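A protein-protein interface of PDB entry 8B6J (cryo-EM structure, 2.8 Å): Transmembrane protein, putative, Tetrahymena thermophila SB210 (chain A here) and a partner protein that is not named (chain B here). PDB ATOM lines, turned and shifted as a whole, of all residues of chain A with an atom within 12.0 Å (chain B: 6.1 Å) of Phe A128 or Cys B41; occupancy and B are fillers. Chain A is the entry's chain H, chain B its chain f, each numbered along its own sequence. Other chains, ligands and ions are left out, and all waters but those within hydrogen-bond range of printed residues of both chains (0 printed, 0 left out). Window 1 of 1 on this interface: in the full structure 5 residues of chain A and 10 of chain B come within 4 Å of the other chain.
Among the printed residues, pairs that only touch across the chains: Tyr A123 with Lys B37, Tyr A127 with Pro B60, Phe A128 with Cys B41, Phe A128 with Lys B44, Phe A128 with Leu B45, Phe A128 with Met B55, Phe A128 with Ser B56 and Ser A129 with Lys B44.
Of the printed residues of chain B, Tyr A123 touches Lys B37 (3.99 Å).
Of the printed residues of chain B, Tyr A127 touches Pro B60.
Of the printed residues of chain B, Phe A128 touches Cys B41 (3.6 Å), Lys B44 (3.9 Å), Leu B45 (3.7 Å), Met B55 (3.8 Å) and Ser B56 (3.9 Å).
Printed residues of chain B within 4 Å of Ser A129: Lys B44.
Of the printed residues of chain A, Lys B37 touches Tyr A123 (3.99 Å).
Gly B39 touches none of the printed residues of chain A.
Cys B41 touches just one residue of chain A: Phe A128.
No residue of chain A comes within 4 Å of Ala B43.
Of chain A, only Phe A128 (3.9 Å) and Ser A129 (3.3 Å) come within 4 Å of Lys B44.
Leu B45 touches one residue of chain A.
Met B55 touches just one residue of chain A: Phe A128 (3.8 Å).
Of chain A, only Phe A128 comes within 4 Å of Ser B56.
No residue of chain A comes within 4 Å of Cys B57.
Pro B60 touches one residue of chain A.
The nearest printed residue of chain B that does not touch Phe A128 is Leu B48 (4.9 Å).
The nearest printed residue of chain B that does not touch Tyr A123 is Pro B60 (7.4 Å).
Of the 17 printed residues of chain B, 7 touch a printed residue of chain A.
Printed residues of chain B that touch a printed residue of chain A: Lys B37, Cys B41, Lys B44, Leu B45, Met B55, Ser B56 and Pro B60.
Hydrophobic or aromatic side chains of chain B within 4 Å of the printed part of chain A: Leu B45, Met B55 and Pro B60.
Along chain B the printed residues that touch a printed residue of chain A span positions 37 to 60.
Among the printed residues, no Asp or Glu carboxylate lies within 4 Å of a Lys or Arg side-chain nitrogen of the other chain.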
ATOM      1  N   ASP A 119     -35.758  -9.735  -9.598  1.00  0.00           N
ATOM      2  CA  ASP A 119     -34.571  -9.013  -9.152  1.00  0.00           C
ATOM      3  C   ASP A 119     -34.456  -9.019  -7.632  1.00  0.00           C
ATOM      4  O   ASP A 119     -33.350  -9.109  -7.092  1.00  0.00           O
ATOM      5  CB  ASP A 119     -34.599  -7.580  -9.680  1.00  0.00           C
ATOM      6  CG  ASP A 119     -34.479  -7.512 -11.190  1.00  0.00           C
ATOM      7  OD1 ASP A 119     -33.788  -8.374 -11.772  1.00  0.00           O
ATOM      8  OD2 ASP A 119     -35.074  -6.596 -11.794  1.00  0.00           O
ATOM      9  N   ASN A 120     -35.581  -8.906  -6.923  1.00  0.00           N
ATOM     10  CA  ASN A 120     -35.534  -8.953  -5.465  1.00  0.00           C
ATOM     11  C   ASN A 120     -35.028 -10.303  -4.980  1.00  0.00           C
ATOM     12  O   ASN A 120     -34.209 -10.373  -4.056  1.00  0.00           O
ATOM     13  CB  ASN A 120     -36.917  -8.661  -4.883  1.00  0.00           C
ATOM     14  CG  ASN A 120     -37.366  -7.239  -5.133  1.00  0.00           C
ATOM     15  OD1 ASN A 120     -36.546  -6.342  -5.327  1.00  0.00           O
ATOM     16  ND2 ASN A 120     -38.675  -7.022  -5.124  1.00  0.00           N
ATOM     17  N   ASN A 121     -35.505 -11.390  -5.589  1.00  0.00           N
ATOM     18  CA  ASN A 121     -35.004 -12.708  -5.212  1.00  0.00           C
ATOM     19  C   ASN A 121     -33.522 -12.841  -5.540  1.00  0.00           C
ATOM     20  O   ASN A 121     -32.755 -13.433  -4.770  1.00  0.00           O
ATOM     21  CB  ASN A 121     -35.807 -13.804  -5.908  1.00  0.00           C
ATOM     22  CG  ASN A 121     -37.263 -13.808  -5.499  1.00  0.00           C
ATOM     23  OD1 ASN A 121     -37.626 -13.279  -4.449  1.00  0.00           O
ATOM     24  ND2 ASN A 121     -38.107 -14.413  -6.323  1.00  0.00           N
ATOM     25  N   CYS A 122     -33.098 -12.295  -6.682  1.00  0.00           N
ATOM     26  CA  CYS A 122     -31.681 -12.326  -7.030  1.00  0.00           C
ATOM     27  C   CYS A 122     -30.842 -11.584  -5.996  1.00  0.00           C
ATOM     28  O   CYS A 122     -29.774 -12.059  -5.592  1.00  0.00           O
ATOM     29  CB  CYS A 122     -31.478 -11.724  -8.419  1.00  0.00           C
ATOM     30  SG  CYS A 122     -29.759 -11.578  -8.922  1.00  0.00           S
ATOM     31  N   TYR A 123     -31.310 -10.414  -5.559  1.00  0.00           N
ATOM     32  CA  TYR A 123     -30.591  -9.660  -4.536  1.00  0.00           C
ATOM     33  C   TYR A 123     -30.528 -10.435  -3.230  1.00  0.00           C
ATOM     34  O   TYR A 123     -29.482 -10.477  -2.573  1.00  0.00           O
ATOM     35  CB  TYR A 123     -31.256  -8.302  -4.316  1.00  0.00           C
ATOM     36  CG  TYR A 123     -30.603  -7.476  -3.230  1.00  0.00           C
ATOM     37  CD1 TYR A 123     -29.482  -6.703  -3.497  1.00  0.00           C
ATOM     38  CD2 TYR A 123     -31.109  -7.468  -1.938  1.00  0.00           C
ATOM     39  CE1 TYR A 123     -28.883  -5.947  -2.511  1.00  0.00           C
ATOM     40  CE2 TYR A 123     -30.515  -6.716  -0.944  1.00  0.00           C
ATOM     41  CZ  TYR A 123     -29.403  -5.958  -1.236  1.00  0.00           C
ATOM     42  OH  TYR A 123     -28.809  -5.207  -0.249  1.00  0.00           O
ATOM     43  N   ASP A 124     -31.640 -11.057  -2.834  1.00  0.00           N
ATOM     44  CA  ASP A 124     -31.627 -11.880  -1.630  1.00  0.00           C
ATOM     45  C   ASP A 124     -30.604 -13.001  -1.753  1.00  0.00           C
ATOM     46  O   ASP A 124     -29.921 -13.340  -0.781  1.00  0.00           O
ATOM     47  CB  ASP A 124     -33.019 -12.452  -1.369  1.00  0.00           C
ATOM     48  CG  ASP A 124     -34.037 -11.380  -1.046  1.00  0.00           C
ATOM     49  OD1 ASP A 124     -33.640 -10.202  -0.912  1.00  0.00           O
ATOM     50  OD2 ASP A 124     -35.234 -11.711  -0.925  1.00  0.00           O
ATOM     51  N   TYR A 125     -30.488 -13.590  -2.944  1.00  0.00           N
ATOM     52  CA  TYR A 125     -29.486 -14.628  -3.164  1.00  0.00           C
ATOM     53  C   TYR A 125     -28.076 -14.074  -3.000  1.00  0.00           C
ATOM     54  O   TYR A 125     -27.240 -14.664  -2.307  1.00  0.00           O
ATOM     55  CB  TYR A 125     -29.662 -15.235  -4.556  1.00  0.00           C
ATOM     56  CG  TYR A 125     -28.581 -16.220  -4.943  1.00  0.00           C
ATOM     57  CD1 TYR A 125     -27.421 -15.796  -5.576  1.00  0.00           C
ATOM     58  CD2 TYR A 125     -28.723 -17.574  -4.679  1.00  0.00           C
ATOM     59  CE1 TYR A 125     -26.432 -16.691  -5.932  1.00  0.00           C
ATOM     60  CE2 TYR A 125     -27.740 -18.477  -5.032  1.00  0.00           C
ATOM     61  CZ  TYR A 125     -26.596 -18.030  -5.658  1.00  0.00           C
ATOM     62  OH  TYR A 125     -25.615 -18.927  -6.011  1.00  0.00           O
ATOM     63  N   PHE A 126     -27.792 -12.933  -3.633  1.00  0.00           N
ATOM     64  CA  PHE A 126     -26.422 -12.426  -3.653  1.00  0.00           C
ATOM     65  C   PHE A 126     -26.016 -11.834  -2.310  1.00  0.00           C
ATOM     66  O   PHE A 126     -24.896 -12.064  -1.840  1.00  0.00           O
ATOM     67  CB  PHE A 126     -26.261 -11.385  -4.761  1.00  0.00           C
ATOM     68  CG  PHE A 126     -25.948 -11.975  -6.105  1.00  0.00           C
ATOM     69  CD1 PHE A 126     -24.742 -12.610  -6.329  1.00  0.00           C
ATOM     70  CD2 PHE A 126     -26.854 -11.888  -7.145  1.00  0.00           C
ATOM     71  CE1 PHE A 126     -24.445 -13.154  -7.560  1.00  0.00           C
ATOM     72  CE2 PHE A 126     -26.560 -12.432  -8.381  1.00  0.00           C
ATOM     73  CZ  PHE A 126     -25.355 -13.065  -8.587  1.00  0.00           C
ATOM     74  N   TYR A 127     -26.902 -11.072  -1.677  1.00  0.00           N
ATOM     75  CA  TYR A 127     -26.576 -10.319  -0.474  1.00  0.00           C
ATOM     76  C   TYR A 127     -27.279 -10.912   0.739  1.00  0.00           C
ATOM     77  O   TYR A 127     -28.443 -11.315   0.658  1.00  0.00           O
ATOM     78  CB  TYR A 127     -26.974  -8.849  -0.626  1.00  0.00           C
ATOM     79  CG  TYR A 127     -26.225  -8.121  -1.714  1.00  0.00           C
ATOM     80  CD1 TYR A 127     -26.608  -8.233  -3.042  1.00  0.00           C
ATOM     81  CD2 TYR A 127     -25.137  -7.315  -1.414  1.00  0.00           C
ATOM     82  CE1 TYR A 127     -25.929  -7.565  -4.039  1.00  0.00           C
ATOM     83  CE2 TYR A 127     -24.451  -6.644  -2.405  1.00  0.00           C
ATOM     84  CZ  TYR A 127     -24.851  -6.773  -3.716  1.00  0.00           C
ATOM     85  OH  TYR A 127     -24.171  -6.107  -4.707  1.00  0.00           O
ATOM     86  N   PHE A 128     -26.562 -10.963   1.858  1.00  0.00           N
ATOM     87  CA  PHE A 128     -27.114 -11.373   3.141  1.00  0.00           C
ATOM     88  C   PHE A 128     -26.937 -10.233   4.132  1.00  0.00           C
ATOM     89  O   PHE A 128     -25.839  -9.684   4.262  1.00  0.00           O
ATOM     90  CB  PHE A 128     -26.436 -12.645   3.657  1.00  0.00           C
ATOM     91  CG  PHE A 128     -24.945 -12.529   3.785  1.00  0.00           C
ATOM     92  CD1 PHE A 128     -24.120 -12.816   2.713  1.00  0.00           C
ATOM     93  CD2 PHE A 128     -24.366 -12.139   4.981  1.00  0.00           C
ATOM     94  CE1 PHE A 128     -22.749 -12.711   2.828  1.00  0.00           C
ATOM     95  CE2 PHE A 128     -22.995 -12.033   5.100  1.00  0.00           C
ATOM     96  CZ  PHE A 128     -22.186 -12.320   4.024  1.00  0.00           C
ATOM     97  N   SER A 129     -28.015  -9.879   4.824  1.00  0.00           N
ATOM     98  CA  SER A 129     -27.998  -8.752   5.750  1.00  0.00           C
ATOM     99  C   SER A 129     -27.597  -7.471   5.030  1.00  0.00           C
ATOM    100  O   SER A 129     -26.413  -7.153   4.928  1.00  0.00           O
ATOM    101  CB  SER A 129     -27.043  -9.020   6.913  1.00  0.00           C
ATOM    102  OG  SER A 129     -27.017  -7.928   7.816  1.00  0.00           O
ATOM    103  N   GLU B  36     -19.853   1.495   5.080  1.00  0.00           N
ATOM    104  CA  GLU B  36     -20.471   0.946   6.281  1.00  0.00           C
ATOM    105  C   GLU B  36     -21.195  -0.359   5.983  1.00  0.00           C
ATOM    106  O   GLU B  36     -21.163  -1.292   6.796  1.00  0.00           O
ATOM    107  CB  GLU B  36     -21.433   1.969   6.882  1.00  0.00           C
ATOM    108  CG  GLU B  36     -20.753   3.233   7.379  1.00  0.00           C
ATOM    109  CD  GLU B  36     -21.734   4.358   7.648  1.00  0.00           C
ATOM    110  OE1 GLU B  36     -22.938   4.179   7.366  1.00  0.00           O
ATOM    111  OE2 GLU B  36     -21.301   5.421   8.140  1.00  0.00           O
ATOM    112  N   LYS B  37     -21.866  -0.445   4.832  1.00  0.00           N
ATOM    113  CA  LYS B  37     -22.516  -1.699   4.469  1.00  0.00           C
ATOM    114  C   LYS B  37     -21.495  -2.820   4.329  1.00  0.00           C
ATOM    115  O   LYS B  37     -21.727  -3.944   4.790  1.00  0.00           O
ATOM    116  CB  LYS B  37     -23.309  -1.532   3.173  1.00  0.00           C
ATOM    117  CG  LYS B  37     -23.984  -2.814   2.704  1.00  0.00           C
ATOM    118  CD  LYS B  37     -24.868  -2.589   1.491  1.00  0.00           C
ATOM    119  CE  LYS B  37     -26.141  -1.842   1.850  1.00  0.00           C
ATOM    120  NZ  LYS B  37     -27.070  -1.739   0.691  1.00  0.00           N
ATOM    121  N   LEU B  38     -20.357  -2.533   3.695  1.00  0.00           N
ATOM    122  CA  LEU B  38     -19.308  -3.540   3.563  1.00  0.00           C
ATOM    123  C   LEU B  38     -18.768  -3.950   4.927  1.00  0.00           C
ATOM    124  O   LEU B  38     -18.526  -5.137   5.178  1.00  0.00           O
ATOM    125  CB  LEU B  38     -18.182  -3.007   2.678  1.00  0.00           C
ATOM    126  CG  LEU B  38     -16.961  -3.912   2.513  1.00  0.00           C
ATOM    127  CD1 LEU B  38     -17.354  -5.255   1.923  1.00  0.00           C
ATOM    128  CD2 LEU B  38     -15.915  -3.232   1.649  1.00  0.00           C
ATOM    129  N   GLY B  39     -18.560  -2.980   5.818  1.00  0.00           N
ATOM    130  CA  GLY B  39     -18.096  -3.312   7.156  1.00  0.00           C
ATOM    131  C   GLY B  39     -19.070  -4.208   7.899  1.00  0.00           C
ATOM    132  O   GLY B  39     -18.668  -5.181   8.543  1.00  0.00           O
ATOM    133  N   ARG B  40     -20.364  -3.894   7.819  1.00  0.00           N
ATOM    134  CA  ARG B  40     -21.366  -4.723   8.479  1.00  0.00           C
ATOM    135  C   ARG B  40     -21.416  -6.118   7.869  1.00  0.00           C
ATOM    136  O   ARG B  40     -21.575  -7.114   8.587  1.00  0.00           O
ATOM    137  CB  ARG B  40     -22.737  -4.050   8.404  1.00  0.00           C
ATOM    138  CG  ARG B  40     -22.878  -2.861   9.339  1.00  0.00           C
ATOM    139  CD  ARG B  40     -24.297  -2.315   9.368  1.00  0.00           C
ATOM    140  NE  ARG B  40     -24.626  -1.552   8.169  1.00  0.00           N
ATOM    141  CZ  ARG B  40     -25.235  -2.045   7.099  1.00  0.00           C
ATOM    142  NH1 ARG B  40     -25.602  -3.316   7.031  1.00  0.00           N
ATOM    143  NH2 ARG B  40     -25.488  -1.242   6.071  1.00  0.00           N
ATOM    144  N   CYS B  41     -21.289  -6.211   6.544  1.00  0.00           N
ATOM    145  CA  CYS B  41     -21.276  -7.519   5.899  1.00  0.00           C
ATOM    146  C   CYS B  41     -20.090  -8.347   6.372  1.00  0.00           C
ATOM    147  O   CYS B  41     -20.231  -9.542   6.662  1.00  0.00           O
ATOM    148  CB  CYS B  41     -21.245  -7.352   4.381  1.00  0.00           C
ATOM    149  SG  CYS B  41     -21.272  -8.904   3.459  1.00  0.00           S
ATOM    150  N   GLU B  42     -18.910  -7.729   6.460  1.00  0.00           N
ATOM    151  CA  GLU B  42     -17.740  -8.449   6.951  1.00  0.00           C
ATOM    152  C   GLU B  42     -17.933  -8.889   8.395  1.00  0.00           C
ATOM    153  O   GLU B  42     -17.579 -10.016   8.762  1.00  0.00           O
ATOM    154  CB  GLU B  42     -16.489  -7.581   6.820  1.00  0.00           C
ATOM    155  CG  GLU B  42     -16.035  -7.366   5.387  1.00  0.00           C
ATOM    156  CD  GLU B  42     -14.670  -6.711   5.302  1.00  0.00           C
ATOM    157  OE1 GLU B  42     -13.956  -6.684   6.325  1.00  0.00           O
ATOM    158  OE2 GLU B  42     -14.313  -6.220   4.211  1.00  0.00           O
ATOM    159  N   ALA B  43     -18.492  -8.014   9.231  1.00  0.00           N
ATOM    160  CA  ALA B  43     -18.740  -8.383  10.621  1.00  0.00           C
ATOM    161  C   ALA B  43     -19.660  -9.594  10.703  1.00  0.00           C
ATOM    162  O   ALA B  43     -19.373 -10.562  11.420  1.00  0.00           O
ATOM    163  CB  ALA B  43     -19.338  -7.197  11.377  1.00  0.00           C
ATOM    164  N   LYS B  44     -20.771  -9.567   9.963  1.00  0.00           N
ATOM    165  CA  LYS B  44     -21.699 -10.692  10.015  1.00  0.00           C
ATOM    166  C   LYS B  44     -21.042 -11.968   9.508  1.00  0.00           C
ATOM    167  O   LYS B  44     -21.208 -13.037  10.107  1.00  0.00           O
ATOM    168  CB  LYS B  44     -22.962 -10.394   9.208  1.00  0.00           C
ATOM    169  CG  LYS B  44     -23.905 -11.591   9.152  1.00  0.00           C
ATOM    170  CD  LYS B  44     -25.277 -11.242   8.614  1.00  0.00           C
ATOM    171  CE  LYS B  44     -26.178 -12.470   8.617  1.00  0.00           C
ATOM    172  NZ  LYS B  44     -27.558 -12.187   8.135  1.00  0.00           N
ATOM    173  N   LEU B  45     -20.294 -11.884   8.406  1.00  0.00           N
ATOM    174  CA  LEU B  45     -19.658 -13.083   7.873  1.00  0.00           C
ATOM    175  C   LEU B  45     -18.650 -13.650   8.864  1.00  0.00           C
ATOM    176  O   LEU B  45     -18.488 -14.871   8.967  1.00  0.00           O
ATOM    177  CB  LEU B  45     -18.991 -12.780   6.534  1.00  0.00           C
ATOM    178  CG  LEU B  45     -18.470 -14.022   5.805  1.00  0.00           C
ATOM    179  CD1 LEU B  45     -18.842 -13.985   4.333  1.00  0.00           C
ATOM    180  CD2 LEU B  45     -16.969 -14.149   5.973  1.00  0.00           C
ATOM    181  N   LYS B  46     -17.959 -12.777   9.602  1.00  0.00           N
ATOM    182  CA  LYS B  46     -17.091 -13.251  10.675  1.00  0.00           C
ATOM    183  C   LYS B  46     -17.896 -13.951  11.762  1.00  0.00           C
ATOM    184  O   LYS B  46     -17.474 -14.987  12.288  1.00  0.00           O
ATOM    185  CB  LYS B  46     -16.300 -12.087  11.268  1.00  0.00           C
ATOM    186  CG  LYS B  46     -15.193 -11.563  10.375  1.00  0.00           C
ATOM    187  CD  LYS B  46     -14.484 -10.376  11.012  1.00  0.00           C
ATOM    188  CE  LYS B  46     -13.368  -9.853  10.124  1.00  0.00           C
ATOM    189  NZ  LYS B  46     -12.720  -8.643  10.694  1.00  0.00           N
ATOM    190  N   LEU B  48     -20.730 -15.619  11.645  1.00  0.00           N
ATOM    191  CA  LEU B  48     -21.263 -16.923  11.275  1.00  0.00           C
ATOM    192  C   LEU B  48     -20.223 -18.017  11.486  1.00  0.00           C
ATOM    193  O   LEU B  48     -19.031 -17.823  11.232  1.00  0.00           O
ATOM    194  CB  LEU B  48     -21.716 -16.915   9.814  1.00  0.00           C
ATOM    195  CG  LEU B  48     -22.868 -15.974   9.462  1.00  0.00           C
ATOM    196  CD1 LEU B  48     -23.163 -16.039   7.974  1.00  0.00           C
ATOM    197  CD2 LEU B  48     -24.111 -16.313  10.268  1.00  0.00           C
ATOM    198  N   MET B  55     -21.464 -17.473   0.333  1.00  0.00           N
ATOM    199  CA  MET B  55     -21.429 -16.199   1.038  1.00  0.00           C
ATOM    200  C   MET B  55     -20.038 -15.583   0.964  1.00  0.00           C
ATOM    201  O   MET B  55     -19.031 -16.259   1.194  1.00  0.00           O
ATOM    202  CB  MET B  55     -21.842 -16.394   2.496  1.00  0.00           C
ATOM    203  CG  MET B  55     -23.297 -16.787   2.679  1.00  0.00           C
ATOM    204  SD  MET B  55     -23.761 -16.918   4.416  1.00  0.00           S
ATOM    205  CE  MET B  55     -25.504 -17.298   4.273  1.00  0.00           C
ATOM    206  N   SER B  56     -19.988 -14.294   0.640  1.00  0.00           N
ATOM    207  CA  SER B  56     -18.722 -13.586   0.522  1.00  0.00           C
ATOM    208  C   SER B  56     -18.982 -12.092   0.621  1.00  0.00           C
ATOM    209  O   SER B  56     -19.989 -11.597   0.108  1.00  0.00           O
ATOM    210  CB  SER B  56     -18.024 -13.913  -0.801  1.00  0.00           C
ATOM    211  OG  SER B  56     -18.801 -13.481  -1.903  1.00  0.00           O
ATOM    212  N   CYS B  57     -18.066 -11.380   1.276  1.00  0.00           N
ATOM    213  CA  CYS B  57     -18.145  -9.927   1.356  1.00  0.00           C
ATOM    214  C   CYS B  57     -17.545  -9.319   0.098  1.00  0.00           C
ATOM    215  O   CYS B  57     -16.665  -8.455   0.171  1.00  0.00           O
ATOM    216  CB  CYS B  57     -17.417  -9.416   2.598  1.00  0.00           C
ATOM    217  SG  CYS B  57     -17.586 -10.488   4.033  1.00  0.00           S
ATOM    218  N   MET B  58     -18.023  -9.763  -1.061  1.00  0.00           N
ATOM    219  CA  MET B  58     -17.469  -9.386  -2.353  1.00  0.00           C
ATOM    220  C   MET B  58     -18.364  -8.414  -3.103  1.00  0.00           C
ATOM    221  O   MET B  58     -17.886  -7.407  -3.632  1.00  0.00           O
ATOM    222  CB  MET B  58     -17.250 -10.649  -3.195  1.00  0.00           C
ATOM    223  CG  MET B  58     -16.485 -10.431  -4.482  1.00  0.00           C
ATOM    224  SD  MET B  58     -16.326 -11.963  -5.414  1.00  0.00           S
ATOM    225  CE  MET B  58     -14.973 -11.551  -6.507  1.00  0.00           C
ATOM    226  N   PRO B  60     -20.807  -6.342  -1.871  1.00  0.00           N
ATOM    227  CA  PRO B  60     -20.761  -5.005  -1.257  1.00  0.00           C
ATOM    228  C   PRO B  60     -19.464  -4.268  -1.536  1.00  0.00           C
ATOM    229  O   PRO B  60     -19.479  -3.056  -1.787  1.00  0.00           O
ATOM    230  CB  PRO B  60     -20.941  -5.302   0.239  1.00  0.00           C
ATOM    231  CG  PRO B  60     -21.573  -6.645   0.296  1.00  0.00           C
ATOM    232  CD  PRO B  60     -21.025  -7.398  -0.870  1.00  0.00           C
